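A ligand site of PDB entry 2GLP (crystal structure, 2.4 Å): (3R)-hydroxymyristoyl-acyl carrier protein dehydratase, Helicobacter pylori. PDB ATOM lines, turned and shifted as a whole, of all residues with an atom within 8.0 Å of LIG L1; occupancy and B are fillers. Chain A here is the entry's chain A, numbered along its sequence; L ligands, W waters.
N1 of LIG L1 is in salt-bridge range of OE2 of Glu 136 (2.7 Å). The side-chain amide nitrogen of Gln 52 lies close to a nitrogen (N2) of LIG L1, 3.1 Å away.
Water W1 bridges NE2 of Gln 52 and N2 of LIG L1.
Val 137 touches LIG L1. Leu 138 touches LIG L1 (CD2 to C4, 3.9 Å). Within 4 Å of LIG L1: Gln 52, Glu 136, Val 137 and Leu 138.
N of Leu 138 sits at hydrogen-bond distance from O of Gln 146, at 2.8 Å. The backbone NH (N) of Glu 136 sits at hydrogen-bond distance from the backbone carbonyl oxygen (O) of Gly 148 (2.8 Å). The backbone NH (N) of Val 137 lies within hydrogen-bond range of the backbone carbonyl oxygen (O) of Gln 52 (2.7 Å).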
ATOM      1  N   GLU A  47     -28.120  22.282 -25.275  1.00  0.00           N
ATOM      2  CA  GLU A  47     -27.043  21.305 -25.276  1.00  0.00           C
ATOM      3  C   GLU A  47     -25.846  21.852 -24.510  1.00  0.00           C
ATOM      4  O   GLU A  47     -25.416  22.982 -24.739  1.00  0.00           O
ATOM      5  CB  GLU A  47     -26.639  20.985 -26.713  1.00  0.00           C
ATOM      6  CG  GLU A  47     -26.038  19.593 -26.900  1.00  0.00           C
ATOM      7  CD  GLU A  47     -25.210  19.476 -28.189  1.00  0.00           C
ATOM      8  OE1 GLU A  47     -25.679  19.934 -29.266  1.00  0.00           O
ATOM      9  OE2 GLU A  47     -24.080  18.927 -28.114  1.00  0.00           O
ATOM     10  N   GLN A  49     -21.918  20.580 -22.836  1.00  0.00           N
ATOM     11  CA  GLN A  49     -20.886  19.570 -22.633  1.00  0.00           C
ATOM     12  C   GLN A  49     -19.686  20.209 -21.963  1.00  0.00           C
ATOM     13  O   GLN A  49     -18.964  20.978 -22.581  1.00  0.00           O
ATOM     14  CB  GLN A  49     -20.447  18.953 -23.962  1.00  0.00           C
ATOM     15  CG  GLN A  49     -19.541  17.735 -23.799  1.00  0.00           C
ATOM     16  CD  GLN A  49     -20.283  16.536 -23.188  1.00  0.00           C
ATOM     17  OE1 GLN A  49     -19.655  15.552 -22.776  1.00  0.00           O
ATOM     18  NE2 GLN A  49     -21.618  16.624 -23.122  1.00  0.00           N
ATOM     19  N   ALA A  50     -19.480  19.853 -20.690  1.00  0.00           N
ATOM     20  CA  ALA A  50     -18.376  20.378 -19.901  1.00  0.00           C
ATOM     21  C   ALA A  50     -17.071  20.514 -20.673  1.00  0.00           C
ATOM     22  O   ALA A  50     -16.633  19.596 -21.363  1.00  0.00           O
ATOM     23  CB  ALA A  50     -18.164  19.501 -18.677  1.00  0.00           C
ATOM     24  N   ASN A  51     -16.450  21.682 -20.536  1.00  0.00           N
ATOM     25  CA  ASN A  51     -15.166  21.993 -21.171  1.00  0.00           C
ATOM     26  C   ASN A  51     -15.135  21.828 -22.674  1.00  0.00           C
ATOM     27  O   ASN A  51     -14.060  21.835 -23.270  1.00  0.00           O
ATOM     28  CB  ASN A  51     -14.041  21.134 -20.568  1.00  0.00           C
ATOM     29  CG  ASN A  51     -14.081  21.091 -19.055  1.00  0.00           C
ATOM     30  OD1 ASN A  51     -14.596  20.150 -18.472  1.00  0.00           O
ATOM     31  ND2 ASN A  51     -13.536  22.115 -18.421  1.00  0.00           N
ATOM     32  N   GLN A  52     -16.290  21.689 -23.315  1.00  0.00           N
ATOM     33  CA  GLN A  52     -16.293  21.537 -24.762  1.00  0.00           C
ATOM     34  C   GLN A  52     -17.185  22.502 -25.495  1.00  0.00           C
ATOM     35  O   GLN A  52     -16.717  23.322 -26.279  1.00  0.00           O
ATOM     36  CB  GLN A  52     -16.666  20.109 -25.162  1.00  0.00           C
ATOM     37  CG  GLN A  52     -15.615  19.082 -24.805  1.00  0.00           C
ATOM     38  CD  GLN A  52     -15.780  17.810 -25.608  1.00  0.00           C
ATOM     39  OE1 GLN A  52     -15.664  16.709 -25.072  1.00  0.00           O
ATOM     40  NE2 GLN A  52     -16.039  17.954 -26.896  1.00  0.00           N
ATOM     41  N   LYS A  53     -18.487  22.402 -25.257  1.00  0.00           N
ATOM     42  CA  LYS A  53     -19.389  23.289 -25.953  1.00  0.00           C
ATOM     43  C   LYS A  53     -20.730  23.469 -25.302  1.00  0.00           C
ATOM     44  O   LYS A  53     -21.082  22.810 -24.330  1.00  0.00           O
ATOM     45  CB  LYS A  53     -19.608  22.789 -27.387  1.00  0.00           C
ATOM     46  CG  LYS A  53     -20.505  21.587 -27.509  1.00  0.00           C
ATOM     47  CD  LYS A  53     -21.412  21.770 -28.715  1.00  0.00           C
ATOM     48  CE  LYS A  53     -21.999  20.455 -29.200  1.00  0.00           C
ATOM     49  NZ  LYS A  53     -22.872  20.659 -30.406  1.00  0.00           N
ATOM     50  N   ILE A  54     -21.479  24.408 -25.881  1.00  0.00           N
ATOM     51  CA  ILE A  54     -22.808  24.725 -25.422  1.00  0.00           C
ATOM     52  C   ILE A  54     -23.600  25.245 -26.600  1.00  0.00           C
ATOM     53  O   ILE A  54     -23.069  25.935 -27.480  1.00  0.00           O
ATOM     54  CB  ILE A  54     -22.754  25.804 -24.296  1.00  0.00           C
ATOM     55  CG1 ILE A  54     -24.165  26.174 -23.842  1.00  0.00           C
ATOM     56  CG2 ILE A  54     -21.995  27.027 -24.782  1.00  0.00           C
ATOM     57  CD1 ILE A  54     -24.208  27.048 -22.600  1.00  0.00           C
ATOM     58  N   LEU A  93     -21.055  28.368 -19.803  1.00  0.00           N
ATOM     59  CA  LEU A  93     -20.319  27.158 -20.113  1.00  0.00           C
ATOM     60  C   LEU A  93     -19.090  27.027 -19.243  1.00  0.00           C
ATOM     61  O   LEU A  93     -18.848  25.985 -18.636  1.00  0.00           O
ATOM     62  CB  LEU A  93     -19.900  27.149 -21.599  1.00  0.00           C
ATOM     63  CG  LEU A  93     -19.131  25.893 -22.055  1.00  0.00           C
ATOM     64  CD1 LEU A  93     -19.983  24.658 -21.761  1.00  0.00           C
ATOM     65  CD2 LEU A  93     -18.789  25.984 -23.528  1.00  0.00           C
ATOM     66  N   LEU A 135     -21.369  27.852 -29.110  1.00  0.00           N
ATOM     67  CA  LEU A 135     -20.022  28.145 -28.617  1.00  0.00           C
ATOM     68  C   LEU A 135     -19.202  26.888 -28.340  1.00  0.00           C
ATOM     69  O   LEU A 135     -19.687  25.936 -27.724  1.00  0.00           O
ATOM     70  CB  LEU A 135     -20.076  28.997 -27.347  1.00  0.00           C
ATOM     71  CG  LEU A 135     -20.361  30.504 -27.426  1.00  0.00           C
ATOM     72  CD1 LEU A 135     -19.368  31.165 -28.365  1.00  0.00           C
ATOM     73  CD2 LEU A 135     -21.790  30.741 -27.906  1.00  0.00           C
ATOM     74  N   GLU A 136     -17.954  26.915 -28.781  1.00  0.00           N
ATOM     75  CA  GLU A 136     -17.029  25.813 -28.588  1.00  0.00           C
ATOM     76  C   GLU A 136     -15.831  26.320 -27.772  1.00  0.00           C
ATOM     77  O   GLU A 136     -15.395  27.457 -27.956  1.00  0.00           O
ATOM     78  CB  GLU A 136     -16.536  25.299 -29.945  1.00  0.00           C
ATOM     79  CG  GLU A 136     -17.632  25.179 -31.018  1.00  0.00           C
ATOM     80  CD  GLU A 136     -18.099  23.760 -31.253  1.00  0.00           C
ATOM     81  OE1 GLU A 136     -18.074  23.315 -32.436  1.00  0.00           O
ATOM     82  OE2 GLU A 136     -18.499  23.084 -30.286  1.00  0.00           O
ATOM     83  N   VAL A 137     -15.318  25.491 -26.880  1.00  0.00           N
ATOM     84  CA  VAL A 137     -14.162  25.860 -26.053  1.00  0.00           C
ATOM     85  C   VAL A 137     -12.850  25.655 -26.816  1.00  0.00           C
ATOM     86  O   VAL A 137     -12.399  24.528 -26.999  1.00  0.00           O
ATOM     87  CB  VAL A 137     -14.118  25.037 -24.771  1.00  0.00           C
ATOM     88  CG1 VAL A 137     -12.881  25.393 -23.967  1.00  0.00           C
ATOM     89  CG2 VAL A 137     -15.384  25.260 -23.957  1.00  0.00           C
ATOM     90  N   LEU A 138     -12.233  26.745 -27.255  1.00  0.00           N
ATOM     91  CA  LEU A 138     -10.975  26.660 -27.992  1.00  0.00           C
ATOM     92  C   LEU A 138      -9.780  26.413 -27.071  1.00  0.00           C
ATOM     93  O   LEU A 138      -8.806  25.758 -27.462  1.00  0.00           O
ATOM     94  CB  LEU A 138     -10.767  27.935 -28.795  1.00  0.00           C
ATOM     95  CG  LEU A 138     -11.889  28.256 -29.791  1.00  0.00           C
ATOM     96  CD1 LEU A 138     -11.662  29.640 -30.381  1.00  0.00           C
ATOM     97  CD2 LEU A 138     -11.938  27.187 -30.881  1.00  0.00           C
ATOM     98  N   LYS A 139      -9.859  26.921 -25.852  1.00  0.00           N
ATOM     99  CA  LYS A 139      -8.774  26.750 -24.889  1.00  0.00           C
ATOM    100  C   LYS A 139      -9.135  27.282 -23.500  1.00  0.00           C
ATOM    101  O   LYS A 139      -9.650  28.397 -23.351  1.00  0.00           O
ATOM    102  CB  LYS A 139      -7.513  27.458 -25.409  1.00  0.00           C
ATOM    103  CG  LYS A 139      -6.403  27.632 -24.396  1.00  0.00           C
ATOM    104  CD  LYS A 139      -5.228  28.403 -24.993  1.00  0.00           C
ATOM    105  CE  LYS A 139      -4.165  28.739 -23.950  1.00  0.00           C
ATOM    106  NZ  LYS A 139      -4.679  29.706 -22.929  1.00  0.00           N
ATOM    107  N   GLN A 146     -11.224  30.678 -23.460  1.00  0.00           N
ATOM    108  CA  GLN A 146     -11.275  31.183 -24.819  1.00  0.00           C
ATOM    109  C   GLN A 146     -12.262  30.370 -25.636  1.00  0.00           C
ATOM    110  O   GLN A 146     -12.053  29.179 -25.878  1.00  0.00           O
ATOM    111  CB  GLN A 146      -9.907  31.127 -25.472  1.00  0.00           C
ATOM    112  CG  GLN A 146      -9.892  31.770 -26.836  1.00  0.00           C
ATOM    113  CD  GLN A 146      -8.537  31.661 -27.505  1.00  0.00           C
ATOM    114  OE1 GLN A 146      -8.183  30.610 -28.075  1.00  0.00           O
ATOM    115  NE2 GLN A 146      -7.750  32.741 -27.417  1.00  0.00           N
ATOM    116  N   GLY A 148     -15.230  30.281 -29.084  1.00  0.00           N
ATOM    117  CA  GLY A 148     -15.500  30.811 -30.396  1.00  0.00           C
ATOM    118  C   GLY A 148     -16.702  30.057 -30.901  1.00  0.00           C
ATOM    119  O   GLY A 148     -17.024  28.987 -30.377  1.00  0.00           O
HETATM  120  C1  LIG L   1     -15.131  21.855 -30.431  1.00  0.00           C
HETATM  121  C2  LIG L   1     -15.144  22.338 -31.774  1.00  0.00           C
HETATM  122  C3  LIG L   1     -14.099  23.138 -32.244  1.00  0.00           C
HETATM  123  C4  LIG L   1     -13.023  23.483 -31.398  1.00  0.00           C
HETATM  124  C5  LIG L   1     -12.996  23.014 -30.063  1.00  0.00           C
HETATM  125  C6  LIG L   1     -14.045  22.202 -29.575  1.00  0.00           C
HETATM  126  C7  LIG L   1     -16.270  20.996 -29.919  1.00  0.00           C
HETATM  127  N1  LIG L   1     -17.267  20.692 -30.691  1.00  0.00           N
HETATM  128  N2  LIG L   1     -16.268  20.532 -28.622  1.00  0.00           N
HETATM  129  C1  LG2 L   2     -17.163  28.954 -37.186  1.00  0.00           C
HETATM  130  C2  LG2 L   2     -18.210  28.264 -37.865  1.00  0.00           C
HETATM  131  C3  LG2 L   2     -18.683  28.735 -39.122  1.00  0.00           C
HETATM  132  C4  LG2 L   2     -18.107  29.876 -39.707  1.00  0.00           C
HETATM  133  C5  LG2 L   2     -17.064  30.573 -39.046  1.00  0.00           C
HETATM  134  C6  LG2 L   2     -16.588  30.115 -37.785  1.00  0.00           C
HETATM  135  C7  LG2 L   2     -16.666  28.459 -35.856  1.00  0.00           C
HETATM  136  N1  LG2 L   2     -17.201  27.386 -35.297  1.00  0.00           N
HETATM  137  N2  LG2 L   2     -15.641  29.129 -35.190  1.00  0.00           N
HETATM  138  O   HOH W   1     -18.567  18.603 -27.870  1.00  0.00           O
